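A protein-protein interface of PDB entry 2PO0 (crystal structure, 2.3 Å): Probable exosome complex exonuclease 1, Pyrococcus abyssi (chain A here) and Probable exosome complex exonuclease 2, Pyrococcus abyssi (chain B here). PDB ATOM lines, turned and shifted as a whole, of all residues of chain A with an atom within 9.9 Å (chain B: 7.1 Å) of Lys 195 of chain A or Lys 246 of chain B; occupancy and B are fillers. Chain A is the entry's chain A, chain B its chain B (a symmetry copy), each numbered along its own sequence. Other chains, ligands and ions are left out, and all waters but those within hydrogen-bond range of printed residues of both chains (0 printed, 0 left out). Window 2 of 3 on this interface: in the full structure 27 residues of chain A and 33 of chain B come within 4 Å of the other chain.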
ATOM      1  N   PRO A 111     -17.619 -21.199  21.770  1.00  0.00           N
ATOM      2  CA  PRO A 111     -18.543 -20.269  22.430  1.00  0.00           C
ATOM      3  C   PRO A 111     -19.857 -20.134  21.687  1.00  0.00           C
ATOM      4  O   PRO A 111     -20.830 -19.593  22.213  1.00  0.00           O
ATOM      5  CB  PRO A 111     -17.786 -18.933  22.363  1.00  0.00           C
ATOM      6  CG  PRO A 111     -16.345 -19.317  22.084  1.00  0.00           C
ATOM      7  CD  PRO A 111     -16.438 -20.498  21.244  1.00  0.00           C
ATOM      8  N   ARG A 156     -25.374 -20.066  18.986  1.00  0.00           N
ATOM      9  CA  ARG A 156     -25.790 -18.779  19.488  1.00  0.00           C
ATOM     10  C   ARG A 156     -25.615 -17.715  18.402  1.00  0.00           C
ATOM     11  O   ARG A 156     -26.236 -16.657  18.454  1.00  0.00           O
ATOM     12  CB  ARG A 156     -24.968 -18.450  20.733  1.00  0.00           C
ATOM     13  CG  ARG A 156     -25.075 -19.549  21.786  1.00  0.00           C
ATOM     14  CD  ARG A 156     -24.558 -19.109  23.138  1.00  0.00           C
ATOM     15  NE  ARG A 156     -23.615 -20.101  23.613  1.00  0.00           N
ATOM     16  CZ  ARG A 156     -23.896 -21.118  24.413  1.00  0.00           C
ATOM     17  NH1 ARG A 156     -25.111 -21.312  24.882  1.00  0.00           N
ATOM     18  NH2 ARG A 156     -22.928 -21.964  24.724  1.00  0.00           N
ATOM     19  N   ASP A 157     -24.769 -18.024  17.418  1.00  0.00           N
ATOM     20  CA  ASP A 157     -24.449 -17.156  16.306  1.00  0.00           C
ATOM     21  C   ASP A 157     -23.534 -17.995  15.450  1.00  0.00           C
ATOM     22  O   ASP A 157     -23.073 -19.052  15.881  1.00  0.00           O
ATOM     23  CB  ASP A 157     -23.666 -15.948  16.812  1.00  0.00           C
ATOM     24  CG  ASP A 157     -23.837 -14.724  15.955  1.00  0.00           C
ATOM     25  OD1 ASP A 157     -24.263 -14.838  14.793  1.00  0.00           O
ATOM     26  OD2 ASP A 157     -23.557 -13.620  16.480  1.00  0.00           O
ATOM     27  N   LEU A 158     -23.294 -17.519  14.233  1.00  0.00           N
ATOM     28  CA  LEU A 158     -22.196 -17.935  13.404  1.00  0.00           C
ATOM     29  C   LEU A 158     -20.879 -17.322  13.868  1.00  0.00           C
ATOM     30  O   LEU A 158     -20.827 -16.332  14.565  1.00  0.00           O
ATOM     31  CB  LEU A 158     -22.467 -17.532  11.950  1.00  0.00           C
ATOM     32  CG  LEU A 158     -23.689 -18.155  11.244  1.00  0.00           C
ATOM     33  CD1 LEU A 158     -23.764 -17.661   9.778  1.00  0.00           C
ATOM     34  CD2 LEU A 158     -23.756 -19.694  11.331  1.00  0.00           C
ATOM     35  N   VAL A 189      -8.758 -12.198  13.526  1.00  0.00           N
ATOM     36  CA  VAL A 189      -9.827 -12.095  14.515  1.00  0.00           C
ATOM     37  C   VAL A 189     -10.988 -13.004  14.097  1.00  0.00           C
ATOM     38  O   VAL A 189     -11.223 -13.194  12.900  1.00  0.00           O
ATOM     39  CB  VAL A 189     -10.259 -10.600  14.732  1.00  0.00           C
ATOM     40  CG1 VAL A 189     -11.330 -10.465  15.792  1.00  0.00           C
ATOM     41  CG2 VAL A 189      -9.026  -9.708  15.101  1.00  0.00           C
ATOM     42  N   ALA A 190     -11.687 -13.594  15.079  1.00  0.00           N
ATOM     43  CA  ALA A 190     -12.957 -14.299  14.822  1.00  0.00           C
ATOM     44  C   ALA A 190     -13.975 -13.761  15.774  1.00  0.00           C
ATOM     45  O   ALA A 190     -13.650 -13.531  16.921  1.00  0.00           O
ATOM     46  CB  ALA A 190     -12.830 -15.812  14.955  1.00  0.00           C
ATOM     47  N   ILE A 191     -15.190 -13.512  15.287  1.00  0.00           N
ATOM     48  CA  ILE A 191     -16.244 -12.987  16.133  1.00  0.00           C
ATOM     49  C   ILE A 191     -17.587 -13.633  15.919  1.00  0.00           C
ATOM     50  O   ILE A 191     -17.854 -14.209  14.877  1.00  0.00           O
ATOM     51  CB  ILE A 191     -16.469 -11.444  15.959  1.00  0.00           C
ATOM     52  CG1 ILE A 191     -16.235 -10.998  14.522  1.00  0.00           C
ATOM     53  CG2 ILE A 191     -15.617 -10.648  16.914  1.00  0.00           C
ATOM     54  CD1 ILE A 191     -17.303 -10.110  14.023  1.00  0.00           C
ATOM     55  N   MET A 192     -18.420 -13.537  16.930  1.00  0.00           N
ATOM     56  CA  MET A 192     -19.828 -13.811  16.830  1.00  0.00           C
ATOM     57  C   MET A 192     -20.418 -12.421  16.708  1.00  0.00           C
ATOM     58  O   MET A 192     -20.451 -11.688  17.681  1.00  0.00           O
ATOM     59  CB  MET A 192     -20.316 -14.516  18.092  1.00  0.00           C
ATOM     60  CG  MET A 192     -19.471 -15.752  18.439  1.00  0.00           C
ATOM     61  SD  MET A 192     -20.143 -16.756  19.780  1.00  0.00           S
ATOM     62  CE  MET A 192     -19.693 -15.833  21.280  1.00  0.00           C
ATOM     63  N   PRO A 193     -20.806 -12.034  15.477  1.00  0.00           N
ATOM     64  CA  PRO A 193     -21.139 -10.661  15.085  1.00  0.00           C
ATOM     65  C   PRO A 193     -22.286 -10.005  15.887  1.00  0.00           C
ATOM     66  O   PRO A 193     -22.120  -8.880  16.396  1.00  0.00           O
ATOM     67  CB  PRO A 193     -21.508 -10.805  13.598  1.00  0.00           C
ATOM     68  CG  PRO A 193     -20.856 -12.019  13.166  1.00  0.00           C
ATOM     69  CD  PRO A 193     -20.892 -12.954  14.325  1.00  0.00           C
ATOM     70  N   LEU A 194     -23.399 -10.723  16.034  1.00  0.00           N
ATOM     71  CA  LEU A 194     -24.581 -10.186  16.647  1.00  0.00           C
ATOM     72  C   LEU A 194     -24.288  -9.512  17.974  1.00  0.00           C
ATOM     73  O   LEU A 194     -24.887  -8.472  18.268  1.00  0.00           O
ATOM     74  CB  LEU A 194     -25.679 -11.247  16.796  1.00  0.00           C
ATOM     75  CG  LEU A 194     -26.419 -11.808  15.575  1.00  0.00           C
ATOM     76  CD1 LEU A 194     -27.692 -12.486  16.024  1.00  0.00           C
ATOM     77  CD2 LEU A 194     -26.761 -10.742  14.529  1.00  0.00           C
ATOM     78  N   LYS A 195     -23.368 -10.067  18.765  1.00  0.00           N
ATOM     79  CA  LYS A 195     -23.084  -9.498  20.081  1.00  0.00           C
ATOM     80  C   LYS A 195     -21.658  -8.995  20.197  1.00  0.00           C
ATOM     81  O   LYS A 195     -21.226  -8.646  21.289  1.00  0.00           O
ATOM     82  CB  LYS A 195     -23.365 -10.501  21.207  1.00  0.00           C
ATOM     83  CG  LYS A 195     -24.776 -10.486  21.784  1.00  0.00           C
ATOM     84  CD  LYS A 195     -25.062 -11.777  22.536  1.00  0.00           C
ATOM     85  CE  LYS A 195     -26.274 -11.642  23.452  1.00  0.00           C
ATOM     86  NZ  LYS A 195     -27.572 -11.273  22.799  1.00  0.00           N
ATOM     87  N   ASN A 196     -20.914  -8.972  19.097  1.00  0.00           N
ATOM     88  CA  ASN A 196     -19.543  -8.441  19.130  1.00  0.00           C
ATOM     89  C   ASN A 196     -18.566  -9.124  20.095  1.00  0.00           C
ATOM     90  O   ASN A 196     -17.774  -8.444  20.786  1.00  0.00           O
ATOM     91  CB  ASN A 196     -19.572  -6.942  19.432  1.00  0.00           C
ATOM     92  CG  ASN A 196     -19.809  -6.130  18.221  1.00  0.00           C
ATOM     93  OD1 ASN A 196     -18.948  -6.054  17.330  1.00  0.00           O
ATOM     94  ND2 ASN A 196     -20.975  -5.521  18.154  1.00  0.00           N
ATOM     95  N   ASP A 197     -18.639 -10.462  20.124  1.00  0.00           N
ATOM     96  CA  ASP A 197     -17.837 -11.278  21.000  1.00  0.00           C
ATOM     97  C   ASP A 197     -16.711 -11.895  20.186  1.00  0.00           C
ATOM     98  O   ASP A 197     -16.960 -12.638  19.241  1.00  0.00           O
ATOM     99  CB  ASP A 197     -18.695 -12.377  21.638  1.00  0.00           C
ATOM    100  CG  ASP A 197     -19.406 -11.924  22.902  1.00  0.00           C
ATOM    101  OD1 ASP A 197     -18.751 -11.309  23.812  1.00  0.00           O
ATOM    102  OD2 ASP A 197     -20.627 -12.221  22.979  1.00  0.00           O
ATOM    103  N   ILE A 198     -15.481 -11.550  20.560  1.00  0.00           N
ATOM    104  CA  ILE A 198     -14.285 -11.998  19.901  1.00  0.00           C
ATOM    105  C   ILE A 198     -13.896 -13.359  20.415  1.00  0.00           C
ATOM    106  O   ILE A 198     -13.574 -13.528  21.582  1.00  0.00           O
ATOM    107  CB  ILE A 198     -13.141 -10.993  20.116  1.00  0.00           C
ATOM    108  CG1 ILE A 198     -13.635  -9.547  19.810  1.00  0.00           C
ATOM    109  CG2 ILE A 198     -11.938 -11.429  19.351  1.00  0.00           C
ATOM    110  CD1 ILE A 198     -12.585  -8.430  20.012  1.00  0.00           C
ATOM    111  N   THR A 199     -13.921 -14.338  19.522  1.00  0.00           N
ATOM    112  CA  THR A 199     -13.676 -15.727  19.898  1.00  0.00           C
ATOM    113  C   THR A 199     -12.306 -16.232  19.434  1.00  0.00           C
ATOM    114  O   THR A 199     -11.809 -17.266  19.914  1.00  0.00           O
ATOM    115  CB  THR A 199     -14.835 -16.645  19.467  1.00  0.00           C
ATOM    116  OG1 THR A 199     -14.782 -16.896  18.073  1.00  0.00           O
ATOM    117  CG2 THR A 199     -16.187 -16.063  19.833  1.00  0.00           C
ATOM    118  N   LEU A 200     -11.673 -15.445  18.568  1.00  0.00           N
ATOM    119  CA  LEU A 200     -10.300 -15.635  18.173  1.00  0.00           C
ATOM    120  C   LEU A 200      -9.555 -14.294  18.116  1.00  0.00           C
ATOM    121  O   LEU A 200     -10.005 -13.317  17.526  1.00  0.00           O
ATOM    122  CB  LEU A 200     -10.202 -16.348  16.818  1.00  0.00           C
ATOM    123  CG  LEU A 200      -8.749 -16.602  16.308  1.00  0.00           C
ATOM    124  CD1 LEU A 200      -8.470 -18.067  15.936  1.00  0.00           C
ATOM    125  CD2 LEU A 200      -8.305 -15.674  15.201  1.00  0.00           C
ATOM    126  N   LEU A 201      -8.394 -14.228  18.717  1.00  0.00           N
ATOM    127  CA  LEU A 201      -7.587 -13.038  18.561  1.00  0.00           C
ATOM    128  C   LEU A 201      -6.146 -13.422  18.686  1.00  0.00           C
ATOM    129  O   LEU A 201      -5.731 -13.877  19.732  1.00  0.00           O
ATOM    130  CB  LEU A 201      -7.926 -11.988  19.622  1.00  0.00           C
ATOM    131  CG  LEU A 201      -7.974 -10.489  19.210  1.00  0.00           C
ATOM    132  CD1 LEU A 201      -7.851  -9.687  20.494  1.00  0.00           C
ATOM    133  CD2 LEU A 201      -6.893 -10.065  18.222  1.00  0.00           C
ATOM    134  N   PHE A 212      -2.174  -2.221  16.960  1.00  0.00           N
ATOM    135  CA  PHE A 212      -2.912  -3.421  17.328  1.00  0.00           C
ATOM    136  C   PHE A 212      -4.418  -3.198  17.292  1.00  0.00           C
ATOM    137  O   PHE A 212      -5.080  -3.863  16.524  1.00  0.00           O
ATOM    138  CB  PHE A 212      -2.511  -3.967  18.693  1.00  0.00           C
ATOM    139  CG  PHE A 212      -3.284  -5.193  19.076  1.00  0.00           C
ATOM    140  CD1 PHE A 212      -4.027  -5.217  20.246  1.00  0.00           C
ATOM    141  CD2 PHE A 212      -3.301  -6.306  18.243  1.00  0.00           C
ATOM    142  CE1 PHE A 212      -4.736  -6.324  20.611  1.00  0.00           C
ATOM    143  CE2 PHE A 212      -4.030  -7.426  18.592  1.00  0.00           C
ATOM    144  CZ  PHE A 212      -4.750  -7.434  19.787  1.00  0.00           C
ATOM    145  N   ILE A 213      -4.920  -2.270  18.114  1.00  0.00           N
ATOM    146  CA  ILE A 213      -6.334  -1.895  18.166  1.00  0.00           C
ATOM    147  C   ILE A 213      -7.016  -1.469  16.827  1.00  0.00           C
ATOM    148  O   ILE A 213      -8.138  -1.934  16.555  1.00  0.00           O
ATOM    149  CB  ILE A 213      -6.630  -0.799  19.299  1.00  0.00           C
ATOM    150  CG1 ILE A 213      -6.350  -1.369  20.708  1.00  0.00           C
ATOM    151  CG2 ILE A 213      -8.049  -0.331  19.237  1.00  0.00           C
ATOM    152  CD1 ILE A 213      -6.871  -2.862  20.980  1.00  0.00           C
ATOM    153  N   VAL A 216      -7.392  -4.833  14.998  1.00  0.00           N
ATOM    154  CA  VAL A 216      -8.508  -5.585  15.598  1.00  0.00           C
ATOM    155  C   VAL A 216      -9.801  -5.019  15.068  1.00  0.00           C
ATOM    156  O   VAL A 216     -10.622  -5.755  14.563  1.00  0.00           O
ATOM    157  CB  VAL A 216      -8.448  -5.611  17.167  1.00  0.00           C
ATOM    158  CG1 VAL A 216      -9.734  -6.200  17.801  1.00  0.00           C
ATOM    159  CG2 VAL A 216      -7.249  -6.420  17.591  1.00  0.00           C
ATOM    160  N   LYS A 217      -9.960  -3.696  15.127  1.00  0.00           N
ATOM    161  CA  LYS A 217     -11.161  -3.052  14.618  1.00  0.00           C
ATOM    162  C   LYS A 217     -11.360  -3.321  13.122  1.00  0.00           C
ATOM    163  O   LYS A 217     -12.477  -3.635  12.706  1.00  0.00           O
ATOM    164  CB  LYS A 217     -11.122  -1.546  14.878  1.00  0.00           C
ATOM    165  CG  LYS A 217     -11.761  -1.072  16.187  1.00  0.00           C
ATOM    166  CD  LYS A 217     -10.922   0.276  16.576  1.00  0.00           C
ATOM    167  CE  LYS A 217     -11.580   0.829  17.916  1.00  0.00           C
ATOM    168  NZ  LYS A 217     -11.082   2.339  18.568  1.00  0.00           N
ATOM    169  N   ILE A 220     -12.438  -6.942  12.422  1.00  0.00           N
ATOM    170  CA  ILE A 220     -13.839  -7.010  12.847  1.00  0.00           C
ATOM    171  C   ILE A 220     -14.765  -6.445  11.754  1.00  0.00           C
ATOM    172  O   ILE A 220     -15.786  -7.052  11.481  1.00  0.00           O
ATOM    173  CB  ILE A 220     -14.070  -6.404  14.279  1.00  0.00           C
ATOM    174  CG1 ILE A 220     -13.388  -7.270  15.334  1.00  0.00           C
ATOM    175  CG2 ILE A 220     -15.546  -6.360  14.643  1.00  0.00           C
ATOM    176  CD1 ILE A 220     -13.328  -6.693  16.699  1.00  0.00           C
ATOM    177  N   LYS A 224     -17.401  -8.972   9.788  1.00  0.00           N
ATOM    178  CA  LYS A 224     -18.832  -8.570   9.602  1.00  0.00           C
ATOM    179  C   LYS A 224     -19.294  -8.620   8.144  1.00  0.00           C
ATOM    180  O   LYS A 224     -20.422  -9.031   7.836  1.00  0.00           O
ATOM    181  CB  LYS A 224     -19.083  -7.186  10.187  1.00  0.00           C
ATOM    182  CG  LYS A 224     -19.162  -7.128  11.719  1.00  0.00           C
ATOM    183  CD  LYS A 224     -19.641  -5.749  12.176  1.00  0.00           C
ATOM    184  CE  LYS A 224     -19.208  -5.384  13.610  1.00  0.00           C
ATOM    185  NZ  LYS A 224     -19.974  -6.123  14.672  1.00  0.00           N
ATOM    186  N   TYR A 227     -19.474 -12.230   7.469  1.00  0.00           N
ATOM    187  CA  TYR A 227     -20.696 -12.678   8.129  1.00  0.00           C
ATOM    188  C   TYR A 227     -21.945 -12.566   7.252  1.00  0.00           C
ATOM    189  O   TYR A 227     -22.807 -13.438   7.303  1.00  0.00           O
ATOM    190  CB  TYR A 227     -20.900 -11.894   9.416  1.00  0.00           C
ATOM    191  CG  TYR A 227     -22.186 -12.218  10.159  1.00  0.00           C
ATOM    192  CD1 TYR A 227     -22.376 -13.480  10.737  1.00  0.00           C
ATOM    193  CD2 TYR A 227     -23.179 -11.249  10.330  1.00  0.00           C
ATOM    194  CE1 TYR A 227     -23.531 -13.776  11.437  1.00  0.00           C
ATOM    195  CE2 TYR A 227     -24.342 -11.532  11.026  1.00  0.00           C
ATOM    196  CZ  TYR A 227     -24.516 -12.817  11.582  1.00  0.00           C
ATOM    197  OH  TYR A 227     -25.670 -13.145  12.283  1.00  0.00           O
ATOM    198  N   LYS B 203     -10.730 -14.360  31.775  1.00  0.00           N
ATOM    199  CA  LYS B 203     -12.071 -13.765  31.864  1.00  0.00           C
ATOM    200  C   LYS B 203     -12.971 -14.813  32.519  1.00  0.00           C
ATOM    201  O   LYS B 203     -13.076 -15.943  31.997  1.00  0.00           O
ATOM    202  CB  LYS B 203     -12.597 -13.389  30.492  1.00  0.00           C
ATOM    203  CG  LYS B 203     -14.071 -13.065  30.442  1.00  0.00           C
ATOM    204  CD  LYS B 203     -14.427 -12.499  29.081  1.00  0.00           C
ATOM    205  CE  LYS B 203     -15.823 -11.975  29.026  1.00  0.00           C
ATOM    206  NZ  LYS B 203     -16.085 -11.439  27.669  1.00  0.00           N
ATOM    207  N   ASN B 206     -17.836 -11.702  33.543  1.00  0.00           N
ATOM    208  CA  ASN B 206     -17.567 -10.400  32.908  1.00  0.00           C
ATOM    209  C   ASN B 206     -16.392  -9.634  33.517  1.00  0.00           C
ATOM    210  O   ASN B 206     -16.227  -8.459  33.253  1.00  0.00           O
ATOM    211  CB  ASN B 206     -18.841  -9.533  32.855  1.00  0.00           C
ATOM    212  CG  ASN B 206     -19.788  -9.962  31.713  1.00  0.00           C
ATOM    213  OD1 ASN B 206     -19.333 -10.192  30.572  1.00  0.00           O
ATOM    214  ND2 ASN B 206     -21.101 -10.102  32.018  1.00  0.00           N
ATOM    215  N   LEU B 208     -12.141  -9.553  34.058  1.00  0.00           N
ATOM    216  CA  LEU B 208     -10.822 -10.111  33.719  1.00  0.00           C
ATOM    217  C   LEU B 208      -9.864 -10.033  34.914  1.00  0.00           C
ATOM    218  O   LEU B 208      -9.815  -9.072  35.596  1.00  0.00           O
ATOM    219  CB  LEU B 208     -10.184  -9.429  32.524  1.00  0.00           C
ATOM    220  CG  LEU B 208     -10.900  -9.127  31.212  1.00  0.00           C
ATOM    221  CD1 LEU B 208      -9.885  -9.006  30.053  1.00  0.00           C
ATOM    222  CD2 LEU B 208     -12.058 -10.020  30.834  1.00  0.00           C
ATOM    223  N   ALA B 244     -15.369 -15.627  24.906  1.00  0.00           N
ATOM    224  CA  ALA B 244     -15.307 -14.509  23.975  1.00  0.00           C
ATOM    225  C   ALA B 244     -14.928 -13.293  24.798  1.00  0.00           C
ATOM    226  O   ALA B 244     -15.192 -13.279  25.994  1.00  0.00           O
ATOM    227  CB  ALA B 244     -16.643 -14.313  23.311  1.00  0.00           C
ATOM    228  N   PHE B 245     -14.275 -12.314  24.162  1.00  0.00           N
ATOM    229  CA  PHE B 245     -13.889 -11.038  24.761  1.00  0.00           C
ATOM    230  C   PHE B 245     -14.564  -9.913  24.011  1.00  0.00           C
ATOM    231  O   PHE B 245     -14.914 -10.063  22.854  1.00  0.00           O
ATOM    232  CB  PHE B 245     -12.360 -10.856  24.733  1.00  0.00           C
ATOM    233  CG  PHE B 245     -11.652 -11.692  25.739  1.00  0.00           C
ATOM    234  CD1 PHE B 245     -11.299 -11.163  26.978  1.00  0.00           C
ATOM    235  CD2 PHE B 245     -11.356 -13.046  25.469  1.00  0.00           C
ATOM    236  CE1 PHE B 245     -10.653 -11.956  27.942  1.00  0.00           C
ATOM    237  CE2 PHE B 245     -10.741 -13.832  26.421  1.00  0.00           C
ATOM    238  CZ  PHE B 245     -10.355 -13.276  27.645  1.00  0.00           C
ATOM    239  N   LYS B 246     -14.753  -8.794  24.702  1.00  0.00           N
ATOM    240  CA  LYS B 246     -15.265  -7.557  24.122  1.00  0.00           C
ATOM    241  C   LYS B 246     -14.059  -6.759  23.698  1.00  0.00           C
ATOM    242  O   LYS B 246     -13.043  -6.811  24.368  1.00  0.00           O
ATOM    243  CB  LYS B 246     -16.030  -6.771  25.183  1.00  0.00           C
ATOM    244  CG  LYS B 246     -17.345  -7.385  25.661  1.00  0.00           C
ATOM    245  CD  LYS B 246     -18.313  -7.509  24.517  1.00  0.00           C
ATOM    246  CE  LYS B 246     -19.575  -8.267  24.886  1.00  0.00           C
ATOM    247  NZ  LYS B 246     -20.569  -7.881  23.846  1.00  0.00           N
ATOM    248  N   LEU B 247     -14.165  -6.019  22.598  1.00  0.00           N
ATOM    249  CA  LEU B 247     -13.096  -5.076  22.221  1.00  0.00           C
ATOM    250  C   LEU B 247     -12.450  -4.312  23.430  1.00  0.00           C
ATOM    251  O   LEU B 247     -11.216  -4.144  23.507  1.00  0.00           O
ATOM    252  CB  LEU B 247     -13.603  -4.062  21.164  1.00  0.00           C
ATOM    253  CG  LEU B 247     -12.747  -3.643  19.950  1.00  0.00           C
ATOM    254  CD1 LEU B 247     -13.100  -2.260  19.512  1.00  0.00           C
ATOM    255  CD2 LEU B 247     -11.235  -3.697  20.159  1.00  0.00           C
ATOM    256  N   GLU B 248     -13.291  -3.830  24.355  1.00  0.00           N
ATOM    257  CA  GLU B 248     -12.823  -2.951  25.429  1.00  0.00           C
ATOM    258  C   GLU B 248     -12.079  -3.736  26.470  1.00  0.00           C
ATOM    259  O   GLU B 248     -11.140  -3.228  27.075  1.00  0.00           O
ATOM    260  CB  GLU B 248     -13.951  -2.116  26.044  1.00  0.00           C
ATOM    261  CG  GLU B 248     -15.340  -2.708  25.867  1.00  0.00           C
ATOM    262  CD  GLU B 248     -15.873  -2.578  24.426  1.00  0.00           C
ATOM    263  OE1 GLU B 248     -15.527  -1.559  23.750  1.00  0.00           O
ATOM    264  OE2 GLU B 248     -16.629  -3.513  23.991  1.00  0.00           O
ATOM    265  N   GLU B 249     -12.479  -4.988  26.658  1.00  0.00           N
ATOM    266  CA  GLU B 249     -11.714  -5.952  27.474  1.00  0.00           C
ATOM    267  C   GLU B 249     -10.370  -6.214  26.852  1.00  0.00           C
ATOM    268  O   GLU B 249      -9.375  -6.372  27.563  1.00  0.00           O
ATOM    269  CB  GLU B 249     -12.481  -7.240  27.628  1.00  0.00           C
ATOM    270  CG  GLU B 249     -13.715  -7.059  28.494  1.00  0.00           C
ATOM    271  CD  GLU B 249     -14.601  -8.290  28.519  1.00  0.00           C
ATOM    272  OE1 GLU B 249     -14.661  -9.029  27.515  1.00  0.00           O
ATOM    273  OE2 GLU B 249     -15.256  -8.519  29.550  1.00  0.00           O
ATOM    274  N   VAL B 250     -10.330  -6.219  25.526  1.00  0.00           N
ATOM    275  CA  VAL B 250      -9.068  -6.307  24.805  1.00  0.00           C
ATOM    276  C   VAL B 250      -8.210  -5.050  24.969  1.00  0.00           C
ATOM    277  O   VAL B 250      -7.046  -5.153  25.340  1.00  0.00           O
ATOM    278  CB  VAL B 250      -9.257  -6.718  23.303  1.00  0.00           C
ATOM    279  CG1 VAL B 250      -7.894  -6.707  22.550  1.00  0.00           C
ATOM    280  CG2 VAL B 250     -10.001  -8.092  23.218  1.00  0.00           C
ATOM    281  N   MET B 251      -8.802  -3.874  24.708  1.00  0.00           N
ATOM    282  CA  MET B 251      -8.203  -2.588  25.049  1.00  0.00           C
ATOM    283  C   MET B 251      -7.662  -2.525  26.488  1.00  0.00           C
ATOM    284  O   MET B 251      -6.530  -2.128  26.710  1.00  0.00           O
ATOM    285  CB  MET B 251      -9.213  -1.471  24.784  1.00  0.00           C
ATOM    286  CG  MET B 251      -9.341  -1.092  23.284  1.00  0.00           C
ATOM    287  SD  MET B 251     -10.916  -0.331  22.742  1.00  0.00           S
ATOM    288  CE  MET B 251     -10.646   1.436  22.940  1.00  0.00           C
ATOM    289  N   TYR B 252      -8.478  -2.927  27.454  1.00  0.00           N
ATOM    290  CA  TYR B 252      -8.103  -2.938  28.870  1.00  0.00           C
ATOM    291  C   TYR B 252      -6.871  -3.823  29.137  1.00  0.00           C
ATOM    292  O   TYR B 252      -5.937  -3.428  29.829  1.00  0.00           O
ATOM    293  CB  TYR B 252      -9.312  -3.372  29.734  1.00  0.00           C
ATOM    294  CG  TYR B 252      -8.898  -3.814  31.116  1.00  0.00           C
ATOM    295  CD1 TYR B 252      -8.672  -5.167  31.425  1.00  0.00           C
ATOM    296  CD2 TYR B 252      -8.686  -2.879  32.102  1.00  0.00           C
ATOM    297  CE1 TYR B 252      -8.240  -5.533  32.688  1.00  0.00           C
ATOM    298  CE2 TYR B 252      -8.271  -3.240  33.345  1.00  0.00           C
ATOM    299  CZ  TYR B 252      -8.058  -4.545  33.641  1.00  0.00           C
ATOM    300  OH  TYR B 252      -7.635  -4.801  34.917  1.00  0.00           O
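O of Lys 195 of chain A is in hydrogen-bond range of NZ of Lys 246 of chain B, 2.7 Å away. OD1 of Asp 197 of chain A lies within salt-bridge range of NZ of Lys 246 of chain B, at 3.9 Å. O of Phe 245 of chain B is in hydrogen-bond range of N of Ile 198 of chain A, at 2.8 Å.
OD1 of Asn 196 of chain A lies within hydrogen-bond range of NZ of Lys 224 of chain A, 2.8 Å away. N of Lys 246 of chain B lies within hydrogen-bond range of OE1 of Glu 249 of chain B (2.8 Å). The backbone carbonyl oxygen of Ala 190 of chain A sits at hydrogen-bond distance from the backbone NH of Thr 199 of chain A (2.7 Å). NZ of Lys 203 of chain B is in hydrogen-bond range of O of Ala 244 of chain B, at 2.6 Å. N of Met 192 of chain A lies within hydrogen-bond range of O of Asp 197 of chain A.
CE of Met 192 of chain A touches CB of Ala 244 of chain B, at 3.97 Å. Asn 196 of chain A touches Phe 245 of chain B. Asn 196 of chain A touches Lys 246 of chain B. Ala 244 of chain B touches Asp 197 of chain A (CB to CB, 3.3 Å). Asp 197 of chain A touches Phe 245 of chain B (CA to O, 3.7 Å). Ile 198 of chain A touches Ala 244 of chain B. Thr 199 of chain A touches Ala 244 of chain B. Phe 212 of chain A touches Val 250 of chain B. Ile 213 of chain A touches Met 251 of chain B. CD2 of Leu 247 of chain B touches CG1 of Val 216 of chain A (3.8 Å).
Of chain B, only Lys 246 comes within 4 Å of Lys 195 of chain A. Of the printed residues of chain B, Phe 212 of chain A touches Val 250. Of the printed residues of chain B, Ile 198 of chain A touches Ala 244, Phe 245 and Leu 247. Printed residues of chain B within 4 Å of Asp 197 of chain A: Ala 244, Phe 245 and Lys 246. Of the printed residues of chain B, Val 216 of chain A touches Leu 247 (3.8 Å). Printed residues of chain A within 4 Å of Phe 245 of chain B: Asn 196, Asp 197 and Ile 198. The nearest residue of chain B that does not touch Lys 195 of chain A is Phe 245 of chain B (6.7 Å). The nearest residue of chain A that does not touch Lys 246 of chain B is Ile 198 of chain A (4.3 Å).
Of the 24 printed residues of chain A, 11 touch a printed residue of chain B. Printed residues of chain A that touch a printed residue of chain B: Met 192, Lys 195, Asn 196, Asp 197, Ile 198, Thr 199, Leu 201, Phe 212, Ile 213, Val 216 and Lys 217. Hydrophobic or aromatic side chains of chain A within 4 Å of the printed part of chain B: Met 192, Ile 198, Leu 201, Phe 212, Ile 213 and Val 216. Of the 12 printed residues of chain B, 6 touch a printed residue of chain A. Hydrophobic or aromatic side chains of chain B within 4 Å of the printed part of chain A: Ala 244, Leu 247, Val 250 and Met 251. Among the printed residues, 16 pairs touch across the chains.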
